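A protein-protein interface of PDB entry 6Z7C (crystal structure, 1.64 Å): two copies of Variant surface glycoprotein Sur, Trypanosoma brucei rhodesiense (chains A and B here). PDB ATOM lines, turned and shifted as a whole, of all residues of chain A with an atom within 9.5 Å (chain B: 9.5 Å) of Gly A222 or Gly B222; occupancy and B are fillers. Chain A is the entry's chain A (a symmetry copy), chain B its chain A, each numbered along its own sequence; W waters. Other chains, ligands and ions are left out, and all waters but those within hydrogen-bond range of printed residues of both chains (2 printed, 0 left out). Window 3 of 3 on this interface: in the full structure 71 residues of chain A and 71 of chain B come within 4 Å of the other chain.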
ATOM      1  N   GLY A 159     -19.025  -1.735  29.641  1.00  0.00           N
ATOM      2  CA  GLY A 159     -18.940  -1.845  28.204  1.00  0.00           C
ATOM      3  C   GLY A 159     -18.461  -0.613  27.474  1.00  0.00           C
ATOM      4  O   GLY A 159     -18.404  -0.625  26.241  1.00  0.00           O
ATOM      5  N   ALA A 160     -18.109   0.452  28.186  1.00  0.00           N
ATOM      6  CA  ALA A 160     -17.680   1.665  27.514  1.00  0.00           C
ATOM      7  C   ALA A 160     -16.212   1.565  27.107  1.00  0.00           C
ATOM      8  O   ALA A 160     -15.433   0.783  27.661  1.00  0.00           O
ATOM      9  CB  ALA A 160     -17.899   2.885  28.413  1.00  0.00           C
ATOM     10  N   THR A 161     -15.847   2.354  26.099  1.00  0.00           N
ATOM     11  CA  THR A 161     -14.444   2.578  25.782  1.00  0.00           C
ATOM     12  C   THR A 161     -13.916   3.869  26.387  1.00  0.00           C
ATOM     13  O   THR A 161     -12.699   4.010  26.556  1.00  0.00           O
ATOM     14  CB  THR A 161     -14.229   2.589  24.260  1.00  0.00           C
ATOM     15  OG1 THR A 161     -15.128   3.522  23.641  1.00  0.00           O
ATOM     16  CG2 THR A 161     -14.472   1.201  23.688  1.00  0.00           C
ATOM     17  N   GLY A 162     -14.798   4.794  26.742  1.00  0.00           N
ATOM     18  CA  GLY A 162     -14.396   5.992  27.445  1.00  0.00           C
ATOM     19  C   GLY A 162     -15.362   6.339  28.556  1.00  0.00           C
ATOM     20  O   GLY A 162     -16.582   6.254  28.382  1.00  0.00           O
ATOM     21  N   GLY A 219     -22.293  14.314  26.861  1.00  0.00           N
ATOM     22  CA  GLY A 219     -21.898  14.624  25.497  1.00  0.00           C
ATOM     23  C   GLY A 219     -20.653  13.874  25.069  1.00  0.00           C
ATOM     24  O   GLY A 219     -19.742  13.682  25.881  1.00  0.00           O
ATOM     25  N   SER A 220     -20.583  13.454  23.806  1.00  0.00           N
ATOM     26  CA  SER A 220     -19.451  12.683  23.317  1.00  0.00           C
ATOM     27  C   SER A 220     -19.056  13.175  21.933  1.00  0.00           C
ATOM     28  O   SER A 220     -19.895  13.627  21.151  1.00  0.00           O
ATOM     29  CB  SER A 220     -19.774  11.180  23.277  1.00  0.00           C
ATOM     30  OG  SER A 220     -18.647  10.410  22.894  1.00  0.00           O
ATOM     31  N   LYS A 221     -17.760  13.089  21.649  1.00  0.00           N
ATOM     32  CA  LYS A 221     -17.221  13.413  20.337  1.00  0.00           C
ATOM     33  C   LYS A 221     -16.015  12.525  20.097  1.00  0.00           C
ATOM     34  O   LYS A 221     -15.202  12.316  21.000  1.00  0.00           O
ATOM     35  CB  LYS A 221     -16.822  14.894  20.236  1.00  0.00           C
ATOM     36  CG  LYS A 221     -16.088  15.273  18.947  1.00  0.00           C
ATOM     37  CD  LYS A 221     -15.473  16.665  19.050  1.00  0.00           C
ATOM     38  CE  LYS A 221     -14.768  17.080  17.772  1.00  0.00           C
ATOM     39  NZ  LYS A 221     -14.107  18.411  17.930  1.00  0.00           N
ATOM     40  N   GLY A 222     -15.906  12.002  18.882  1.00  0.00           N
ATOM     41  CA  GLY A 222     -14.744  11.199  18.560  1.00  0.00           C
ATOM     42  C   GLY A 222     -14.692   9.919  19.368  1.00  0.00           C
ATOM     43  O   GLY A 222     -15.707   9.248  19.591  1.00  0.00           O
ATOM     44  N   ASN A 223     -13.484   9.578  19.826  1.00  0.00           N
ATOM     45  CA  ASN A 223     -13.193   8.318  20.508  1.00  0.00           C
ATOM     46  C   ASN A 223     -12.581   8.635  21.870  1.00  0.00           C
ATOM     47  O   ASN A 223     -11.358   8.531  22.055  1.00  0.00           O
ATOM     48  CB  ASN A 223     -12.264   7.458  19.651  1.00  0.00           C
ATOM     49  CG  ASN A 223     -11.836   6.172  20.336  1.00  0.00           C
ATOM     50  OD1 ASN A 223     -12.587   5.578  21.107  1.00  0.00           O
ATOM     51  ND2 ASN A 223     -10.616   5.734  20.048  1.00  0.00           N
ATOM     52  N   PRO A 224     -13.396   9.044  22.842  1.00  0.00           N
ATOM     53  CA  PRO A 224     -12.856   9.325  24.179  1.00  0.00           C
ATOM     54  C   PRO A 224     -12.422   8.045  24.877  1.00  0.00           C
ATOM     55  O   PRO A 224     -13.117   7.027  24.834  1.00  0.00           O
ATOM     56  CB  PRO A 224     -14.033   9.987  24.905  1.00  0.00           C
ATOM     57  CG  PRO A 224     -15.250   9.455  24.206  1.00  0.00           C
ATOM     58  CD  PRO A 224     -14.846   9.295  22.762  1.00  0.00           C
ATOM     59  N   THR A 225     -11.249   8.097  25.507  1.00  0.00           N
ATOM     60  CA  THR A 225     -10.707   6.955  26.237  1.00  0.00           C
ATOM     61  C   THR A 225     -10.054   7.470  27.513  1.00  0.00           C
ATOM     62  O   THR A 225     -10.201   8.639  27.884  1.00  0.00           O
ATOM     63  CB  THR A 225      -9.692   6.162  25.396  1.00  0.00           C
ATOM     64  OG1 THR A 225      -8.565   6.993  25.091  1.00  0.00           O
ATOM     65  CG2 THR A 225     -10.315   5.657  24.102  1.00  0.00           C
ATOM     66  N   SER A 228      -8.029  10.662  27.374  1.00  0.00           N
ATOM     67  CA  SER A 228      -8.695  11.961  27.285  1.00  0.00           C
ATOM     68  C   SER A 228      -8.565  12.729  28.605  1.00  0.00           C
ATOM     69  O   SER A 228      -9.547  13.082  29.255  1.00  0.00           O
ATOM     70  CB  SER A 228     -10.155  11.759  26.896  1.00  0.00           C
ATOM     71  OG  SER A 228     -10.249  10.980  25.711  1.00  0.00           O
ATOM     72  N   CYS A 236     -13.472  15.555  29.662  1.00  0.00           N
ATOM     73  CA  CYS A 236     -12.339  14.704  29.311  1.00  0.00           C
ATOM     74  C   CYS A 236     -12.064  14.848  27.818  1.00  0.00           C
ATOM     75  O   CYS A 236     -12.890  14.447  26.993  1.00  0.00           O
ATOM     76  CB  CYS A 236     -12.635  13.253  29.686  1.00  0.00           C
ATOM     77  SG  CYS A 236     -12.937  12.980  31.456  1.00  0.00           S
ATOM     78  N   ASP A 238      -8.875  14.810  24.536  1.00  0.00           N
ATOM     79  CA  ASP A 238      -7.519  14.627  24.032  1.00  0.00           C
ATOM     80  C   ASP A 238      -7.569  14.584  22.511  1.00  0.00           C
ATOM     81  O   ASP A 238      -8.635  14.440  21.906  1.00  0.00           O
ATOM     82  CB  ASP A 238      -6.858  13.364  24.605  1.00  0.00           C
ATOM     83  CG  ASP A 238      -7.292  12.088  23.899  1.00  0.00           C
ATOM     84  OD1 ASP A 238      -8.498  11.913  23.637  1.00  0.00           O
ATOM     85  OD2 ASP A 238      -6.411  11.253  23.610  1.00  0.00           O
ATOM     86  N   GLY A 239      -6.394  14.716  21.898  1.00  0.00           N
ATOM     87  CA  GLY A 239      -6.298  14.711  20.452  1.00  0.00           C
ATOM     88  C   GLY A 239      -6.592  16.063  19.838  1.00  0.00           C
ATOM     89  O   GLY A 239      -7.433  16.810  20.345  1.00  0.00           O
ATOM     90  N   PHE A 246     -15.791  21.191  23.285  1.00  0.00           N
ATOM     91  CA  PHE A 246     -15.215  19.953  22.753  1.00  0.00           C
ATOM     92  C   PHE A 246     -14.237  20.248  21.614  1.00  0.00           C
ATOM     93  O   PHE A 246     -14.316  19.667  20.528  1.00  0.00           O
ATOM     94  CB  PHE A 246     -16.311  18.984  22.294  1.00  0.00           C
ATOM     95  CG  PHE A 246     -16.997  18.253  23.420  1.00  0.00           C
ATOM     96  CD1 PHE A 246     -16.724  18.564  24.745  1.00  0.00           C
ATOM     97  CD2 PHE A 246     -17.902  17.237  23.150  1.00  0.00           C
ATOM     98  CE1 PHE A 246     -17.341  17.886  25.777  1.00  0.00           C
ATOM     99  CE2 PHE A 246     -18.524  16.553  24.179  1.00  0.00           C
ATOM    100  CZ  PHE A 246     -18.242  16.878  25.496  1.00  0.00           C
ATOM    101  N   GLY A 248     -11.200  19.432  21.256  1.00  0.00           N
ATOM    102  CA  GLY A 248     -10.325  18.330  20.924  1.00  0.00           C
ATOM    103  C   GLY A 248     -10.986  17.289  20.041  1.00  0.00           C
ATOM    104  O   GLY A 248     -12.195  17.289  19.802  1.00  0.00           O
ATOM    105  N   ALA A 249     -10.150  16.373  19.545  1.00  0.00           N
ATOM    106  CA  ALA A 249     -10.632  15.341  18.632  1.00  0.00           C
ATOM    107  C   ALA A 249     -11.545  14.352  19.345  1.00  0.00           C
ATOM    108  O   ALA A 249     -12.540  13.888  18.772  1.00  0.00           O
ATOM    109  CB  ALA A 249      -9.449  14.614  17.994  1.00  0.00           C
ATOM    110  N   ASN A 250     -11.219  14.021  20.592  1.00  0.00           N
ATOM    111  CA  ASN A 250     -11.999  13.103  21.411  1.00  0.00           C
ATOM    112  C   ASN A 250     -12.433  13.826  22.674  1.00  0.00           C
ATOM    113  O   ASN A 250     -11.616  14.487  23.326  1.00  0.00           O
ATOM    114  CB  ASN A 250     -11.181  11.864  21.770  1.00  0.00           C
ATOM    115  CG  ASN A 250     -10.497  11.270  20.579  1.00  0.00           C
ATOM    116  OD1 ASN A 250     -11.110  11.099  19.527  1.00  0.00           O
ATOM    117  ND2 ASN A 250      -9.212  10.970  20.721  1.00  0.00           N
ATOM    118  N   ALA A 251     -13.709  13.696  23.022  1.00  0.00           N
ATOM    119  CA  ALA A 251     -14.240  14.406  24.173  1.00  0.00           C
ATOM    120  C   ALA A 251     -15.384  13.612  24.782  1.00  0.00           C
ATOM    121  O   ALA A 251     -16.176  12.994  24.064  1.00  0.00           O
ATOM    122  CB  ALA A 251     -14.713  15.810  23.789  1.00  0.00           C
ATOM    123  N   LEU A 252     -15.452  13.630  26.110  1.00  0.00           N
ATOM    124  CA  LEU A 252     -16.557  13.048  26.856  1.00  0.00           C
ATOM    125  C   LEU A 252     -16.778  13.882  28.105  1.00  0.00           C
ATOM    126  O   LEU A 252     -15.819  14.263  28.781  1.00  0.00           O
ATOM    127  CB  LEU A 252     -16.281  11.590  27.239  1.00  0.00           C
ATOM    128  CG  LEU A 252     -17.350  10.884  28.075  1.00  0.00           C
ATOM    129  CD1 LEU A 252     -18.694  10.884  27.357  1.00  0.00           C
ATOM    130  CD2 LEU A 252     -16.909   9.465  28.380  1.00  0.00           C
ATOM    131  N   GLY B 159     -20.378  21.252  20.779  1.00  0.00           N
ATOM    132  CA  GLY B 159     -19.366  20.573  20.003  1.00  0.00           C
ATOM    133  C   GLY B 159     -19.463  19.067  19.964  1.00  0.00           C
ATOM    134  O   GLY B 159     -18.605  18.422  19.352  1.00  0.00           O
ATOM    135  N   ALA B 160     -20.478  18.478  20.587  1.00  0.00           N
ATOM    136  CA  ALA B 160     -20.580  17.030  20.600  1.00  0.00           C
ATOM    137  C   ALA B 160     -21.202  16.523  19.302  1.00  0.00           C
ATOM    138  O   ALA B 160     -21.901  17.247  18.586  1.00  0.00           O
ATOM    139  CB  ALA B 160     -21.403  16.559  21.802  1.00  0.00           C
ATOM    140  N   THR B 161     -20.911  15.262  18.987  1.00  0.00           N
ATOM    141  CA  THR B 161     -21.640  14.554  17.946  1.00  0.00           C
ATOM    142  C   THR B 161     -22.749  13.680  18.510  1.00  0.00           C
ATOM    143  O   THR B 161     -23.688  13.339  17.783  1.00  0.00           O
ATOM    144  CB  THR B 161     -20.682  13.699  17.100  1.00  0.00           C
ATOM    145  OG1 THR B 161     -19.898  12.849  17.951  1.00  0.00           O
ATOM    146  CG2 THR B 161     -19.756  14.596  16.294  1.00  0.00           C
ATOM    147  N   GLY B 162     -22.677  13.338  19.790  1.00  0.00           N
ATOM    148  CA  GLY B 162     -23.751  12.623  20.443  1.00  0.00           C
ATOM    149  C   GLY B 162     -24.024  13.165  21.828  1.00  0.00           C
ATOM    150  O   GLY B 162     -23.092  13.459  22.586  1.00  0.00           O
ATOM    151  N   GLY B 219     -20.403   7.570  30.201  1.00  0.00           N
ATOM    152  CA  GLY B 219     -19.751   6.508  29.454  1.00  0.00           C
ATOM    153  C   GLY B 219     -20.048   6.577  27.970  1.00  0.00           C
ATOM    154  O   GLY B 219     -21.170   6.920  27.583  1.00  0.00           O
ATOM    155  N   SER B 220     -19.073   6.245  27.124  1.00  0.00           N
ATOM    156  CA  SER B 220     -19.248   6.328  25.683  1.00  0.00           C
ATOM    157  C   SER B 220     -18.629   5.107  25.020  1.00  0.00           C
ATOM    158  O   SER B 220     -17.641   4.548  25.504  1.00  0.00           O
ATOM    159  CB  SER B 220     -18.625   7.615  25.117  1.00  0.00           C
ATOM    160  OG  SER B 220     -18.873   7.754  23.728  1.00  0.00           O
ATOM    161  N   LYS B 221     -19.233   4.695  23.910  1.00  0.00           N
ATOM    162  CA  LYS B 221     -18.714   3.611  23.090  1.00  0.00           C
ATOM    163  C   LYS B 221     -19.086   3.900  21.647  1.00  0.00           C
ATOM    164  O   LYS B 221     -20.207   4.331  21.365  1.00  0.00           O
ATOM    165  CB  LYS B 221     -19.279   2.250  23.524  1.00  0.00           C
ATOM    166  CG  LYS B 221     -18.917   1.083  22.602  1.00  0.00           C
ATOM    167  CD  LYS B 221     -19.744  -0.157  22.927  1.00  0.00           C
ATOM    168  CE  LYS B 221     -19.381  -1.340  22.049  1.00  0.00           C
ATOM    169  NZ  LYS B 221     -20.261  -2.513  22.336  1.00  0.00           N
ATOM    170  N   GLY B 222     -18.144   3.668  20.742  1.00  0.00           N
ATOM    171  CA  GLY B 222     -18.451   3.856  19.339  1.00  0.00           C
ATOM    172  C   GLY B 222     -18.738   5.305  19.006  1.00  0.00           C
ATOM    173  O   GLY B 222     -18.076   6.229  19.493  1.00  0.00           O
ATOM    174  N   ASN B 223     -19.756   5.510  18.166  1.00  0.00           N
ATOM    175  CA  ASN B 223     -20.111   6.816  17.612  1.00  0.00           C
ATOM    176  C   ASN B 223     -21.570   7.107  17.957  1.00  0.00           C
ATOM    177  O   ASN B 223     -22.461   6.973  17.105  1.00  0.00           O
ATOM    178  CB  ASN B 223     -19.867   6.833  16.103  1.00  0.00           C
ATOM    179  CG  ASN B 223     -20.306   8.126  15.440  1.00  0.00           C
ATOM    180  OD1 ASN B 223     -20.228   9.203  16.026  1.00  0.00           O
ATOM    181  ND2 ASN B 223     -20.768   8.019  14.199  1.00  0.00           N
ATOM    182  N   PRO B 224     -21.854   7.488  19.203  1.00  0.00           N
ATOM    183  CA  PRO B 224     -23.238   7.814  19.569  1.00  0.00           C
ATOM    184  C   PRO B 224     -23.692   9.108  18.910  1.00  0.00           C
ATOM    185  O   PRO B 224     -22.954  10.094  18.864  1.00  0.00           O
ATOM    186  CB  PRO B 224     -23.179   7.955  21.094  1.00  0.00           C
ATOM    187  CG  PRO B 224     -21.756   8.339  21.378  1.00  0.00           C
ATOM    188  CD  PRO B 224     -20.931   7.615  20.344  1.00  0.00           C
ATOM    189  N   THR B 225     -24.913   9.091  18.377  1.00  0.00           N
ATOM    190  CA  THR B 225     -25.495  10.261  17.726  1.00  0.00           C
ATOM    191  C   THR B 225     -26.968  10.336  18.105  1.00  0.00           C
ATOM    192  O   THR B 225     -27.443   9.613  18.987  1.00  0.00           O
ATOM    193  CB  THR B 225     -25.334  10.209  16.198  1.00  0.00           C
ATOM    194  OG1 THR B 225     -26.051   9.084  15.675  1.00  0.00           O
ATOM    195  CG2 THR B 225     -23.870  10.110  15.795  1.00  0.00           C
ATOM    196  N   SER B 228     -28.989   7.141  18.236  1.00  0.00           N
ATOM    197  CA  SER B 228     -28.832   6.208  19.351  1.00  0.00           C
ATOM    198  C   SER B 228     -30.066   6.233  20.259  1.00  0.00           C
ATOM    199  O   SER B 228     -29.997   6.536  21.448  1.00  0.00           O
ATOM    200  CB  SER B 228     -27.562   6.546  20.123  1.00  0.00           C
ATOM    201  OG  SER B 228     -26.445   6.590  19.245  1.00  0.00           O
ATOM    202  N   CYS B 236     -28.408   5.742  25.753  1.00  0.00           N
ATOM    203  CA  CYS B 236     -28.663   5.962  24.333  1.00  0.00           C
ATOM    204  C   CYS B 236     -27.798   4.999  23.527  1.00  0.00           C
ATOM    205  O   CYS B 236     -26.568   5.110  23.538  1.00  0.00           O
ATOM    206  CB  CYS B 236     -28.370   7.415  23.964  1.00  0.00           C
ATOM    207  SG  CYS B 236     -29.384   8.635  24.850  1.00  0.00           S
ATOM    208  N   ASP B 238     -27.464   2.504  19.704  1.00  0.00           N
ATOM    209  CA  ASP B 238     -27.923   2.044  18.400  1.00  0.00           C
ATOM    210  C   ASP B 238     -26.781   1.302  17.719  1.00  0.00           C
ATOM    211  O   ASP B 238     -25.623   1.379  18.137  1.00  0.00           O
ATOM    212  CB  ASP B 238     -28.436   3.200  17.528  1.00  0.00           C
ATOM    213  CG  ASP B 238     -27.319   3.985  16.857  1.00  0.00           C
ATOM    214  OD1 ASP B 238     -26.311   4.302  17.518  1.00  0.00           O
ATOM    215  OD2 ASP B 238     -27.461   4.289  15.655  1.00  0.00           O
ATOM    216  N   GLY B 239     -27.127   0.573  16.659  1.00  0.00           N
ATOM    217  CA  GLY B 239     -26.142  -0.198  15.926  1.00  0.00           C
ATOM    218  C   GLY B 239     -25.859  -1.544  16.560  1.00  0.00           C
ATOM    219  O   GLY B 239     -25.877  -1.672  17.787  1.00  0.00           O
ATOM    220  N   PHE B 246     -23.764  -1.565  27.441  1.00  0.00           N
ATOM    221  CA  PHE B 246     -23.431  -0.980  26.140  1.00  0.00           C
ATOM    222  C   PHE B 246     -23.312  -2.064  25.066  1.00  0.00           C
ATOM    223  O   PHE B 246     -22.327  -2.134  24.326  1.00  0.00           O
ATOM    224  CB  PHE B 246     -22.146  -0.147  26.218  1.00  0.00           C
ATOM    225  CG  PHE B 246     -22.331   1.210  26.850  1.00  0.00           C
ATOM    226  CD1 PHE B 246     -23.544   1.574  27.418  1.00  0.00           C
ATOM    227  CD2 PHE B 246     -21.294   2.131  26.852  1.00  0.00           C
ATOM    228  CE1 PHE B 246     -23.718   2.821  27.984  1.00  0.00           C
ATOM    229  CE2 PHE B 246     -21.462   3.383  27.416  1.00  0.00           C
ATOM    230  CZ  PHE B 246     -22.678   3.729  27.983  1.00  0.00           C
ATOM    231  N   GLY B 248     -24.792  -2.366  22.285  1.00  0.00           N
ATOM    232  CA  GLY B 248     -24.831  -1.866  20.929  1.00  0.00           C
ATOM    233  C   GLY B 248     -23.500  -1.306  20.463  1.00  0.00           C
ATOM    234  O   GLY B 248     -22.552  -1.118  21.227  1.00  0.00           O
ATOM    235  N   ALA B 249     -23.443  -1.032  19.157  1.00  0.00           N
ATOM    236  CA  ALA B 249     -22.208  -0.541  18.553  1.00  0.00           C
ATOM    237  C   ALA B 249     -21.883   0.870  19.024  1.00  0.00           C
ATOM    238  O   ALA B 249     -20.711   1.207  19.240  1.00  0.00           O
ATOM    239  CB  ALA B 249     -22.320  -0.584  17.029  1.00  0.00           C
ATOM    240  N   ASN B 250     -22.907   1.704  19.187  1.00  0.00           N
ATOM    241  CA  ASN B 250     -22.762   3.078  19.647  1.00  0.00           C
ATOM    242  C   ASN B 250     -23.582   3.256  20.913  1.00  0.00           C
ATOM    243  O   ASN B 250     -24.747   2.845  20.964  1.00  0.00           O
ATOM    244  CB  ASN B 250     -23.228   4.063  18.577  1.00  0.00           C
ATOM    245  CG  ASN B 250     -22.653   3.752  17.231  1.00  0.00           C
ATOM    246  OD1 ASN B 250     -21.455   3.504  17.103  1.00  0.00           O
ATOM    247  ND2 ASN B 250     -23.503   3.741  16.211  1.00  0.00           N
ATOM    248  N   ALA B 251     -22.980   3.871  21.926  1.00  0.00           N
ATOM    249  CA  ALA B 251     -23.654   4.027  23.204  1.00  0.00           C
ATOM    250  C   ALA B 251     -23.155   5.284  23.896  1.00  0.00           C
ATOM    251  O   ALA B 251     -21.969   5.620  23.820  1.00  0.00           O
ATOM    252  CB  ALA B 251     -23.435   2.805  24.099  1.00  0.00           C
ATOM    253  N   LEU B 252     -24.076   5.976  24.561  1.00  0.00           N
ATOM    254  CA  LEU B 252     -23.756   7.123  25.398  1.00  0.00           C
ATOM    255  C   LEU B 252     -24.731   7.149  26.562  1.00  0.00           C
ATOM    256  O   LEU B 252     -25.933   6.943  26.375  1.00  0.00           O
ATOM    257  CB  LEU B 252     -23.834   8.438  24.617  1.00  0.00           C
ATOM    258  CG  LEU B 252     -23.570   9.724  25.404  1.00  0.00           C
ATOM    259  CD1 LEU B 252     -22.188   9.697  26.047  1.00  0.00           C
ATOM    260  CD2 LEU B 252     -23.708  10.924  24.488  1.00  0.00           C
HETATM  261  O   HOH W   1     -17.599  11.832  16.585  1.00  0.00           O
HETATM  262  O   HOH W   2     -15.355   3.050  20.828  1.00  0.00           O
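O of Ser A220 is in hydrogen-bond range of N of Thr B161, 2.9 Å away. The backbone carbonyl oxygen (O) of Gly B162 is in hydrogen-bond range of the backbone NH (N) of Ser A220 (2.8 Å). The backbone carbonyl oxygen of Ser B220 lies within hydrogen-bond range of the backbone NH of Thr A161 (2.9 Å). O of Gly A162 sits at hydrogen-bond distance from N of Ser B220 (2.8 Å). The side-chain hydroxyl of Ser A220 lies within hydrogen-bond range of the side-chain hydroxyl of Ser B220 (2.8 Å).
The backbone carbonyl oxygen of Pro B224 lies close to the backbone NH of Gly B162 (3.4 Å). O of Phe B246 sits at hydrogen-bond distance from NZ of Lys B221, 2.9 Å away. The backbone NH (N) of Cys B236 lies within hydrogen-bond range of the backbone carbonyl oxygen (O) of Leu B252. O of Pro A224 sits close to N of Gly A162. NZ of Lys A221 lies within hydrogen-bond range of O of Gly A248 (2.9 Å). The backbone carbonyl oxygen of Leu A252 lies within hydrogen-bond range of the backbone NH of Cys A236, at 2.8 Å.
Among the printed residues, merely in contact across the chains: Gly A162 with Gly B219 (3.4 Å), Gly A219 with Gly B162 (3.4 Å), Ala A160 with Ser B220 (3.4 Å), Ser A220 with Ala B160 (3.4 Å), Lys A221 with Gly B159 (3.6 Å), Gly A159 with Lys B221 (3.6 Å), Thr A161 with Lys B221 (3.6 Å), Lys A221 with Thr B161 (3.6 Å), Ala A160 with Phe B246 (3.7 Å), Phe A246 with Ala B160 (3.7 Å), Gly A159 with Phe B246 (3.8 Å), Phe A246 with Gly B159 (3.8 Å), Gly A222 with Gly B222 (3.8 Å), Leu A252 with Leu B252 (3.9 Å), Ser A220 with Pro B224 (3.95 Å), Pro A224 with Ser B220 (3.95 Å), Ser A220 with Leu B252 (3.96 Å) and Leu A252 with Ser B220 (3.96 Å).
Gly A222 touches just one residue of chain B: Gly B222 (3.8 Å). Of the printed residues of chain B, Pro A224 touches Ser B220. Thr A225 touches none of the printed residues of chain B. Gly A248 touches none of the printed residues of chain B. Printed residues of chain A within 4 Å of Thr B161: Ser A220 and Lys A221. Printed residues of chain A within 4 Å of Gly B219: Gly A162 (3.4 Å). Of the printed residues of chain A, Lys B221 touches Gly A159 and Thr A161. Of chain A, only Gly A222 comes within 4 Å of Gly B222. The nearest residue of chain A that does not touch Gly B222 is Thr A161 (4.2 Å).
Of the 21 printed residues of chain B, 11 touch a printed residue of chain A. Along chain A the printed residues that touch a printed residue of chain B span positions 159 to 252. Among the printed residues, no Asp or Glu carboxylate lies within 4 Å of a Lys or Arg side-chain nitrogen of the other chain.
Gly A159 touches Lys B221, and with the chains exchanged Lys A221 touches Gly B159. Ala A160 touches Phe B246, and with the chains exchanged Phe A246 touches Ala B160. Thr A161 touches Ser B220, and with the chains exchanged Ser A220 touches Thr B161. Leu B252 touches its own counterpart, Leu A252. 21 positions are printed for both chains. Of the 23 pairs that touch across the chains among the printed residues, 23 have their exchanged pair printed and touching as well.
Water W2 lies within hydrogen-bond range of N of Gly B222 (2.9 Å) and OG1 of Thr A161 (2.9 Å). Water W1 bridges N of Gly A222 (2.9 Å) and OG1 of Thr B161 (2.9 Å).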
